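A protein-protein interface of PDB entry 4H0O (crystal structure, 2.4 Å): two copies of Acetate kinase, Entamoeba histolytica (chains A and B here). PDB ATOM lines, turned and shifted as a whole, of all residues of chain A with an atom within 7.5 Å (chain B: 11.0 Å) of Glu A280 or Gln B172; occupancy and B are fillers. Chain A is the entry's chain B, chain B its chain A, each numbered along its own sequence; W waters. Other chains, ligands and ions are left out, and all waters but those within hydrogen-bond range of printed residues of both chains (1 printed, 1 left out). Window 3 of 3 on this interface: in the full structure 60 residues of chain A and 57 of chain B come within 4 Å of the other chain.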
ATOM      1  N   ILE A 268      33.310  19.506  20.775  1.00  0.00           N
ATOM      2  CA  ILE A 268      31.989  19.222  20.211  1.00  0.00           C
ATOM      3  C   ILE A 268      30.929  20.212  20.709  1.00  0.00           C
ATOM      4  O   ILE A 268      30.172  20.778  19.913  1.00  0.00           O
ATOM      5  CB  ILE A 268      31.539  17.779  20.525  1.00  0.00           C
ATOM      6  CG1 ILE A 268      32.400  16.765  19.764  1.00  0.00           C
ATOM      7  CG2 ILE A 268      30.083  17.584  20.161  1.00  0.00           C
ATOM      8  CD1 ILE A 268      32.255  15.324  20.263  1.00  0.00           C
ATOM      9  N   LYS A 272      30.925  22.412  17.559  1.00  0.00           N
ATOM     10  CA  LYS A 272      30.154  21.543  16.677  1.00  0.00           C
ATOM     11  C   LYS A 272      28.742  21.266  17.188  1.00  0.00           C
ATOM     12  O   LYS A 272      28.173  20.209  16.911  1.00  0.00           O
ATOM     13  CB  LYS A 272      30.895  20.221  16.451  1.00  0.00           C
ATOM     14  CG  LYS A 272      32.021  20.308  15.433  1.00  0.00           C
ATOM     15  CD  LYS A 272      33.352  20.603  16.105  1.00  0.00           C
ATOM     16  CE  LYS A 272      34.495  20.569  15.103  1.00  0.00           C
ATOM     17  NZ  LYS A 272      35.729  21.200  15.648  1.00  0.00           N
ATOM     18  N   GLY A 274      24.881  23.518  18.799  1.00  0.00           N
ATOM     19  CA  GLY A 274      23.956  24.603  18.529  1.00  0.00           C
ATOM     20  C   GLY A 274      23.326  24.543  17.150  1.00  0.00           C
ATOM     21  O   GLY A 274      23.008  23.460  16.651  1.00  0.00           O
ATOM     22  N   LEU A 275      23.154  25.710  16.533  1.00  0.00           N
ATOM     23  CA  LEU A 275      22.564  25.805  15.202  1.00  0.00           C
ATOM     24  C   LEU A 275      23.312  24.945  14.182  1.00  0.00           C
ATOM     25  O   LEU A 275      22.693  24.277  13.353  1.00  0.00           O
ATOM     26  CB  LEU A 275      22.528  27.263  14.745  1.00  0.00           C
ATOM     27  CG  LEU A 275      21.578  28.188  15.506  1.00  0.00           C
ATOM     28  CD1 LEU A 275      21.776  29.640  15.088  1.00  0.00           C
ATOM     29  CD2 LEU A 275      20.133  27.769  15.286  1.00  0.00           C
ATOM     30  N   LEU A 276      24.639  24.959  14.251  1.00  0.00           N
ATOM     31  CA  LEU A 276      25.462  24.189  13.320  1.00  0.00           C
ATOM     32  C   LEU A 276      25.219  22.690  13.463  1.00  0.00           C
ATOM     33  O   LEU A 276      25.011  21.989  12.470  1.00  0.00           O
ATOM     34  CB  LEU A 276      26.948  24.500  13.530  1.00  0.00           C
ATOM     35  CG  LEU A 276      27.948  23.726  12.667  1.00  0.00           C
ATOM     36  CD1 LEU A 276      27.679  23.960  11.191  1.00  0.00           C
ATOM     37  CD2 LEU A 276      29.380  24.114  13.014  1.00  0.00           C
ATOM     38  N   GLY A 277      25.230  22.208  14.702  1.00  0.00           N
ATOM     39  CA  GLY A 277      25.105  20.787  14.972  1.00  0.00           C
ATOM     40  C   GLY A 277      23.757  20.164  14.650  1.00  0.00           C
ATOM     41  O   GLY A 277      23.693  18.998  14.254  1.00  0.00           O
ATOM     42  N   VAL A 278      22.678  20.921  14.831  1.00  0.00           N
ATOM     43  CA  VAL A 278      21.337  20.390  14.591  1.00  0.00           C
ATOM     44  C   VAL A 278      20.911  20.526  13.129  1.00  0.00           C
ATOM     45  O   VAL A 278      20.354  19.594  12.549  1.00  0.00           O
ATOM     46  CB  VAL A 278      20.288  21.068  15.489  1.00  0.00           C
ATOM     47  CG1 VAL A 278      18.919  20.431  15.286  1.00  0.00           C
ATOM     48  CG2 VAL A 278      20.700  20.973  16.946  1.00  0.00           C
ATOM     49  N   SER A 279      21.167  21.692  12.540  1.00  0.00           N
ATOM     50  CA  SER A 279      20.809  21.939  11.144  1.00  0.00           C
ATOM     51  C   SER A 279      21.643  21.087  10.196  1.00  0.00           C
ATOM     52  O   SER A 279      21.171  20.707   9.123  1.00  0.00           O
ATOM     53  CB  SER A 279      20.995  23.415  10.785  1.00  0.00           C
ATOM     54  OG  SER A 279      22.370  23.743  10.654  1.00  0.00           O
ATOM     55  N   GLU A 280      22.882  20.801  10.601  1.00  0.00           N
ATOM     56  CA  GLU A 280      23.844  20.067   9.777  1.00  0.00           C
ATOM     57  C   GLU A 280      24.131  20.805   8.472  1.00  0.00           C
ATOM     58  O   GLU A 280      24.505  20.189   7.474  1.00  0.00           O
ATOM     59  CB  GLU A 280      23.358  18.638   9.493  1.00  0.00           C
ATOM     60  CG  GLU A 280      23.164  17.782  10.738  1.00  0.00           C
ATOM     61  CD  GLU A 280      22.596  16.407  10.423  1.00  0.00           C
ATOM     62  OE1 GLU A 280      22.269  16.149   9.243  1.00  0.00           O
ATOM     63  OE2 GLU A 280      22.478  15.583  11.356  1.00  0.00           O
ATOM     64  N   LEU A 281      23.962  22.126   8.492  1.00  0.00           N
ATOM     65  CA  LEU A 281      24.127  22.954   7.301  1.00  0.00           C
ATOM     66  C   LEU A 281      25.059  24.137   7.546  1.00  0.00           C
ATOM     67  O   LEU A 281      26.143  24.218   6.968  1.00  0.00           O
ATOM     68  CB  LEU A 281      22.771  23.477   6.824  1.00  0.00           C
ATOM     69  CG  LEU A 281      22.818  24.440   5.634  1.00  0.00           C
ATOM     70  CD1 LEU A 281      22.879  23.677   4.324  1.00  0.00           C
ATOM     71  CD2 LEU A 281      21.633  25.394   5.647  1.00  0.00           C
ATOM     72  N   SER A 282      24.623  25.055   8.404  1.00  0.00           N
ATOM     73  CA  SER A 282      25.362  26.288   8.664  1.00  0.00           C
ATOM     74  C   SER A 282      25.254  26.698  10.131  1.00  0.00           C
ATOM     75  O   SER A 282      24.352  26.253  10.847  1.00  0.00           O
ATOM     76  CB  SER A 282      24.830  27.419   7.775  1.00  0.00           C
ATOM     77  OG  SER A 282      25.533  28.631   7.991  1.00  0.00           O
ATOM     78  N   SER A 283      26.178  27.550  10.570  1.00  0.00           N
ATOM     79  CA  SER A 283      26.113  28.135  11.903  1.00  0.00           C
ATOM     80  C   SER A 283      25.332  29.444  11.854  1.00  0.00           C
ATOM     81  O   SER A 283      25.014  30.027  12.891  1.00  0.00           O
ATOM     82  CB  SER A 283      27.519  28.392  12.450  1.00  0.00           C
ATOM     83  OG  SER A 283      28.185  29.400  11.708  1.00  0.00           O
ATOM     84  N   ILE A 288      20.058  28.978   7.422  1.00  0.00           N
ATOM     85  CA  ILE A 288      19.110  27.981   7.915  1.00  0.00           C
ATOM     86  C   ILE A 288      17.687  28.295   7.457  1.00  0.00           C
ATOM     87  O   ILE A 288      16.990  27.425   6.933  1.00  0.00           O
ATOM     88  CB  ILE A 288      19.162  27.880   9.458  1.00  0.00           C
ATOM     89  CG1 ILE A 288      20.478  27.235   9.896  1.00  0.00           C
ATOM     90  CG2 ILE A 288      17.987  27.080   9.991  1.00  0.00           C
ATOM     91  CD1 ILE A 288      20.711  27.244  11.394  1.00  0.00           C
ATOM     92  N   LYS A 298      18.405  19.890   3.217  1.00  0.00           N
ATOM     93  CA  LYS A 298      18.519  19.833   4.674  1.00  0.00           C
ATOM     94  C   LYS A 298      17.424  20.626   5.394  1.00  0.00           C
ATOM     95  O   LYS A 298      17.627  21.120   6.504  1.00  0.00           O
ATOM     96  CB  LYS A 298      19.905  20.315   5.113  1.00  0.00           C
ATOM     97  CG  LYS A 298      21.040  19.433   4.616  1.00  0.00           C
ATOM     98  CD  LYS A 298      22.396  19.942   5.064  1.00  0.00           C
ATOM     99  CE  LYS A 298      23.480  18.930   4.733  1.00  0.00           C
ATOM    100  NZ  LYS A 298      23.132  17.583   5.264  1.00  0.00           N
ATOM    101  N   THR A 301      16.143  19.256   9.022  1.00  0.00           N
ATOM    102  CA  THR A 301      17.100  19.507  10.096  1.00  0.00           C
ATOM    103  C   THR A 301      17.251  20.994  10.403  1.00  0.00           C
ATOM    104  O   THR A 301      17.483  21.379  11.552  1.00  0.00           O
ATOM    105  CB  THR A 301      18.481  18.888   9.794  1.00  0.00           C
ATOM    106  OG1 THR A 301      18.806  19.092   8.415  1.00  0.00           O
ATOM    107  CG2 THR A 301      18.464  17.397  10.094  1.00  0.00           C
ATOM    108  N   CYS A 302      17.132  21.827   9.375  1.00  0.00           N
ATOM    109  CA  CYS A 302      17.153  23.272   9.564  1.00  0.00           C
ATOM    110  C   CYS A 302      15.896  23.742  10.292  1.00  0.00           C
ATOM    111  O   CYS A 302      15.947  24.655  11.114  1.00  0.00           O
ATOM    112  CB  CYS A 302      17.301  23.995   8.225  1.00  0.00           C
ATOM    113  SG  CYS A 302      18.958  23.883   7.506  1.00  0.00           S
ATOM    114  N   LEU A 304      14.262  21.862  12.389  1.00  0.00           N
ATOM    115  CA  LEU A 304      14.445  21.373  13.751  1.00  0.00           C
ATOM    116  C   LEU A 304      15.352  22.313  14.539  1.00  0.00           C
ATOM    117  O   LEU A 304      15.070  22.647  15.689  1.00  0.00           O
ATOM    118  CB  LEU A 304      15.032  19.959  13.742  1.00  0.00           C
ATOM    119  CG  LEU A 304      15.330  19.365  15.122  1.00  0.00           C
ATOM    120  CD1 LEU A 304      14.057  19.257  15.951  1.00  0.00           C
ATOM    121  CD2 LEU A 304      16.023  18.008  15.016  1.00  0.00           C
ATOM    122  N   ALA A 305      16.439  22.742  13.906  1.00  0.00           N
ATOM    123  CA  ALA A 305      17.380  23.655  14.539  1.00  0.00           C
ATOM    124  C   ALA A 305      16.701  24.962  14.938  1.00  0.00           C
ATOM    125  O   ALA A 305      16.935  25.476  16.032  1.00  0.00           O
ATOM    126  CB  ALA A 305      18.562  23.920  13.623  1.00  0.00           C
ATOM    127  N   GLN B 163       9.414  16.106  19.135  1.00  0.00           N
ATOM    128  CA  GLN B 163      10.849  15.985  18.879  1.00  0.00           C
ATOM    129  C   GLN B 163      11.634  17.217  19.328  1.00  0.00           C
ATOM    130  O   GLN B 163      12.669  17.100  19.984  1.00  0.00           O
ATOM    131  CB  GLN B 163      11.101  15.731  17.388  1.00  0.00           C
ATOM    132  CG  GLN B 163      12.574  15.612  17.016  1.00  0.00           C
ATOM    133  CD  GLN B 163      12.789  15.325  15.540  1.00  0.00           C
ATOM    134  OE1 GLN B 163      11.952  15.657  14.700  1.00  0.00           O
ATOM    135  NE2 GLN B 163      13.918  14.705  15.220  1.00  0.00           N
ATOM    136  N   ARG B 166      12.237  17.333  22.912  1.00  0.00           N
ATOM    137  CA  ARG B 166      13.060  16.224  23.403  1.00  0.00           C
ATOM    138  C   ARG B 166      14.522  16.371  22.991  1.00  0.00           C
ATOM    139  O   ARG B 166      15.400  15.702  23.539  1.00  0.00           O
ATOM    140  CB  ARG B 166      12.541  14.879  22.874  1.00  0.00           C
ATOM    141  CG  ARG B 166      11.126  14.508  23.291  1.00  0.00           C
ATOM    142  CD  ARG B 166      10.769  13.100  22.831  1.00  0.00           C
ATOM    143  NE  ARG B 166      11.476  12.076  23.599  1.00  0.00           N
ATOM    144  CZ  ARG B 166      11.852  10.896  23.113  1.00  0.00           C
ATOM    145  NH1 ARG B 166      11.603  10.581  21.851  1.00  0.00           N
ATOM    146  NH2 ARG B 166      12.489  10.032  23.890  1.00  0.00           N
ATOM    147  N   THR B 167      14.773  17.243  22.021  1.00  0.00           N
ATOM    148  CA  THR B 167      16.085  17.339  21.390  1.00  0.00           C
ATOM    149  C   THR B 167      16.992  18.384  22.038  1.00  0.00           C
ATOM    150  O   THR B 167      16.625  19.557  22.156  1.00  0.00           O
ATOM    151  CB  THR B 167      15.953  17.665  19.885  1.00  0.00           C
ATOM    152  OG1 THR B 167      15.196  16.635  19.239  1.00  0.00           O
ATOM    153  CG2 THR B 167      17.323  17.769  19.231  1.00  0.00           C
ATOM    154  N   TYR B 168      18.179  17.955  22.452  1.00  0.00           N
ATOM    155  CA  TYR B 168      19.214  18.890  22.875  1.00  0.00           C
ATOM    156  C   TYR B 168      20.025  19.376  21.669  1.00  0.00           C
ATOM    157  O   TYR B 168      20.243  18.633  20.711  1.00  0.00           O
ATOM    158  CB  TYR B 168      20.127  18.239  23.909  1.00  0.00           C
ATOM    159  CG  TYR B 168      19.432  17.956  25.215  1.00  0.00           C
ATOM    160  CD1 TYR B 168      19.231  18.966  26.142  1.00  0.00           C
ATOM    161  CD2 TYR B 168      18.976  16.680  25.521  1.00  0.00           C
ATOM    162  CE1 TYR B 168      18.596  18.717  27.339  1.00  0.00           C
ATOM    163  CE2 TYR B 168      18.339  16.420  26.716  1.00  0.00           C
ATOM    164  CZ  TYR B 168      18.154  17.443  27.622  1.00  0.00           C
ATOM    165  OH  TYR B 168      17.520  17.200  28.816  1.00  0.00           O
ATOM    166  N   ALA B 169      20.477  20.623  21.721  1.00  0.00           N
ATOM    167  CA  ALA B 169      21.197  21.216  20.599  1.00  0.00           C
ATOM    168  C   ALA B 169      22.625  20.670  20.462  1.00  0.00           C
ATOM    169  O   ALA B 169      23.602  21.416  20.581  1.00  0.00           O
ATOM    170  CB  ALA B 169      21.209  22.734  20.719  1.00  0.00           C
ATOM    171  N   ILE B 170      22.734  19.368  20.201  1.00  0.00           N
ATOM    172  CA  ILE B 170      24.022  18.706  19.987  1.00  0.00           C
ATOM    173  C   ILE B 170      23.972  17.945  18.658  1.00  0.00           C
ATOM    174  O   ILE B 170      22.888  17.588  18.192  1.00  0.00           O
ATOM    175  CB  ILE B 170      24.368  17.742  21.152  1.00  0.00           C
ATOM    176  CG1 ILE B 170      23.307  16.647  21.294  1.00  0.00           C
ATOM    177  CG2 ILE B 170      24.525  18.513  22.456  1.00  0.00           C
ATOM    178  CD1 ILE B 170      23.523  15.726  22.498  1.00  0.00           C
ATOM    179  N   PRO B 171      25.136  17.694  18.037  1.00  0.00           N
ATOM    180  CA  PRO B 171      25.084  17.048  16.721  1.00  0.00           C
ATOM    181  C   PRO B 171      24.863  15.540  16.831  1.00  0.00           C
ATOM    182  O   PRO B 171      25.078  14.962  17.903  1.00  0.00           O
ATOM    183  CB  PRO B 171      26.481  17.312  16.159  1.00  0.00           C
ATOM    184  CG  PRO B 171      27.353  17.308  17.381  1.00  0.00           C
ATOM    185  CD  PRO B 171      26.525  17.963  18.464  1.00  0.00           C
ATOM    186  N   GLN B 172      24.434  14.914  15.737  1.00  0.00           N
ATOM    187  CA  GLN B 172      24.401  13.458  15.664  1.00  0.00           C
ATOM    188  C   GLN B 172      25.846  12.966  15.741  1.00  0.00           C
ATOM    189  O   GLN B 172      26.761  13.682  15.337  1.00  0.00           O
ATOM    190  CB  GLN B 172      23.729  12.989  14.365  1.00  0.00           C
ATOM    191  CG  GLN B 172      22.264  13.429  14.197  1.00  0.00           C
ATOM    192  CD  GLN B 172      21.307  12.757  15.176  1.00  0.00           C
ATOM    193  OE1 GLN B 172      21.711  11.936  16.005  1.00  0.00           O
ATOM    194  NE2 GLN B 172      20.025  13.108  15.080  1.00  0.00           N
ATOM    195  N   PRO B 173      26.067  11.744  16.255  1.00  0.00           N
ATOM    196  CA  PRO B 173      25.078  10.759  16.713  1.00  0.00           C
ATOM    197  C   PRO B 173      24.601  10.997  18.142  1.00  0.00           C
ATOM    198  O   PRO B 173      23.655  10.341  18.574  1.00  0.00           O
ATOM    199  CB  PRO B 173      25.862   9.448  16.656  1.00  0.00           C
ATOM    200  CG  PRO B 173      27.262   9.862  16.993  1.00  0.00           C
ATOM    201  CD  PRO B 173      27.445  11.228  16.372  1.00  0.00           C
ATOM    202  N   TYR B 174      25.243  11.911  18.859  1.00  0.00           N
ATOM    203  CA  TYR B 174      24.927  12.140  20.266  1.00  0.00           C
ATOM    204  C   TYR B 174      23.498  12.648  20.464  1.00  0.00           C
ATOM    205  O   TYR B 174      22.880  12.406  21.504  1.00  0.00           O
ATOM    206  CB  TYR B 174      25.946  13.105  20.876  1.00  0.00           C
ATOM    207  CG  TYR B 174      27.368  12.780  20.473  1.00  0.00           C
ATOM    208  CD1 TYR B 174      28.091  11.803  21.142  1.00  0.00           C
ATOM    209  CD2 TYR B 174      27.978  13.438  19.414  1.00  0.00           C
ATOM    210  CE1 TYR B 174      29.386  11.495  20.772  1.00  0.00           C
ATOM    211  CE2 TYR B 174      29.272  13.136  19.036  1.00  0.00           C
ATOM    212  CZ  TYR B 174      29.970  12.165  19.719  1.00  0.00           C
ATOM    213  OH  TYR B 174      31.260  11.861  19.348  1.00  0.00           O
ATOM    214  N   GLN B 175      22.972  13.333  19.452  1.00  0.00           N
ATOM    215  CA  GLN B 175      21.622  13.890  19.506  1.00  0.00           C
ATOM    216  C   GLN B 175      20.552  12.822  19.742  1.00  0.00           C
ATOM    217  O   GLN B 175      19.682  12.986  20.597  1.00  0.00           O
ATOM    218  CB  GLN B 175      21.315  14.667  18.222  1.00  0.00           C
ATOM    219  CG  GLN B 175      19.967  15.374  18.232  1.00  0.00           C
ATOM    220  CD  GLN B 175      19.663  16.074  16.921  1.00  0.00           C
ATOM    221  OE1 GLN B 175      18.559  15.963  16.386  1.00  0.00           O
ATOM    222  NE2 GLN B 175      20.640  16.807  16.401  1.00  0.00           N
ATOM    223  N   SER B 176      20.622  11.730  18.987  1.00  0.00           N
ATOM    224  CA  SER B 176      19.648  10.647  19.121  1.00  0.00           C
ATOM    225  C   SER B 176      19.948   9.727  20.300  1.00  0.00           C
ATOM    226  O   SER B 176      19.057   9.026  20.785  1.00  0.00           O
ATOM    227  CB  SER B 176      19.554   9.836  17.826  1.00  0.00           C
ATOM    228  OG  SER B 176      18.837  10.548  16.837  1.00  0.00           O
ATOM    229  N   GLN B 177      21.200   9.721  20.753  1.00  0.00           N
ATOM    230  CA  GLN B 177      21.591   8.906  21.901  1.00  0.00           C
ATOM    231  C   GLN B 177      21.044   9.478  23.209  1.00  0.00           C
ATOM    232  O   GLN B 177      20.682   8.730  24.119  1.00  0.00           O
ATOM    233  CB  GLN B 177      23.119   8.767  21.978  1.00  0.00           C
ATOM    234  CG  GLN B 177      23.743   7.916  20.861  1.00  0.00           C
ATOM    235  CD  GLN B 177      25.267   7.983  20.835  1.00  0.00           C
ATOM    236  OE1 GLN B 177      25.890   8.655  21.659  1.00  0.00           O
ATOM    237  NE2 GLN B 177      25.871   7.286  19.879  1.00  0.00           N
ATOM    238  N   TYR B 178      20.978  10.805  23.297  1.00  0.00           N
ATOM    239  CA  TYR B 178      20.589  11.467  24.539  1.00  0.00           C
ATOM    240  C   TYR B 178      19.337  12.328  24.392  1.00  0.00           C
ATOM    241  O   TYR B 178      19.349  13.516  24.720  1.00  0.00           O
ATOM    242  CB  TYR B 178      21.744  12.313  25.078  1.00  0.00           C
ATOM    243  CG  TYR B 178      23.043  11.551  25.216  1.00  0.00           C
ATOM    244  CD1 TYR B 178      23.184  10.556  26.173  1.00  0.00           C
ATOM    245  CD2 TYR B 178      24.131  11.832  24.398  1.00  0.00           C
ATOM    246  CE1 TYR B 178      24.365   9.854  26.306  1.00  0.00           C
ATOM    247  CE2 TYR B 178      25.320  11.137  24.528  1.00  0.00           C
ATOM    248  CZ  TYR B 178      25.429  10.150  25.486  1.00  0.00           C
ATOM    249  OH  TYR B 178      26.605   9.451  25.624  1.00  0.00           O
ATOM    250  N   LEU B 179      18.260  11.726  23.898  1.00  0.00           N
ATOM    251  CA  LEU B 179      16.972  12.406  23.839  1.00  0.00           C
ATOM    252  C   LEU B 179      16.405  12.529  25.250  1.00  0.00           C
ATOM    253  O   LEU B 179      16.722  11.722  26.128  1.00  0.00           O
ATOM    254  CB  LEU B 179      15.992  11.642  22.943  1.00  0.00           C
ATOM    255  CG  LEU B 179      16.315  11.632  21.447  1.00  0.00           C
ATOM    256  CD1 LEU B 179      15.394  10.692  20.686  1.00  0.00           C
ATOM    257  CD2 LEU B 179      16.214  13.035  20.874  1.00  0.00           C
HETATM  258  O   HOH W   1      23.954  16.543  13.641  1.00  0.00           O
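The backbone carbonyl oxygen of Ala B169 lies within hydrogen-bond range of the backbone NH of Gly A274 (3.0 Å).
The side-chain amide oxygen (OE1) of Gln B172 sits at hydrogen-bond distance from the backbone NH (N) of Ser B176.
OG1 of Thr B167 lies within hydrogen-bond range of O of Gln B163, 2.7 Å away.
NE2 of Gln B175 lies within hydrogen-bond range of O of Ile B170 (3.0 Å).
OE1 of Gln B175 sits at hydrogen-bond distance from NE2 of Gln B172 (3.5 Å).
Among the printed residues, pairs that only touch across the chains: Lys A272 with Pro B171 (3.1 Å), Gly A277 with Pro B171 (3.4 Å), Leu A304 with Gln B175 (3.5 Å), Glu A280 with Gln B172 (3.6 Å), Val A278 with Ala B169 (3.7 Å), Ile A268 with Tyr B174 (3.7 Å), Ile A268 with Pro B171 (3.9 Å) and Leu A304 with Gln B163 (3.9 Å).
Printed residues of chain B within 4 Å of Ile A268: Pro B171 and Tyr B174.
Of the printed residues of chain B, Gly A274 touches Ala B169 (3.0 Å).
Of chain B, only Ala B169 (3.7 Å) comes within 4 Å of Val A278.
Ser A279 touches none of the printed residues of chain B.
Of chain B, only Gln B172 (3.6 Å) comes within 4 Å of Glu A280.
No residue of chain B comes within 4 Å of Leu A281.
Thr A301 touches none of the printed residues of chain B.
Printed residues of chain A within 4 Å of Gln B163: Leu A304 (3.9 Å).
Ile B170 touches none of the printed residues of chain A.
Gln B172 touches just one residue of chain A: Glu A280 (3.6 Å).
Printed residues of chain A within 4 Å of Tyr B174: Ile A268 (3.7 Å).
Ser B176 touches none of the printed residues of chain A.
The nearest residue of chain A that does not touch Gln B172 is Gly A277 (4.4 Å).
Of the 15 printed residues of chain B, 6 touch a printed residue of chain A.
Hydrophobic or aromatic side chains of chain B that line the printed part of chain A: Ala B169, Pro B171 and Tyr B174.
Hydrophobic or aromatic side chains of chain A that line the printed part of chain B: Ile A268, Val A278 and Leu A304.
Among the printed residues, no Asp or Glu carboxylate lies within 4 Å of a Lys or Arg side-chain nitrogen of the other chain.
No position is printed for both chains.
Of the 9 pairs that touch across the chains among the printed residues, none has its exchanged pair printed and touching as well.
Water W1 lies within hydrogen-bond range of the backbone carbonyl oxygen of Gly A277 (2.5 Å), the backbone NH of Gln B172 (2.7 Å) and the side-chain carboxylate of Glu A280 (2.9 Å).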
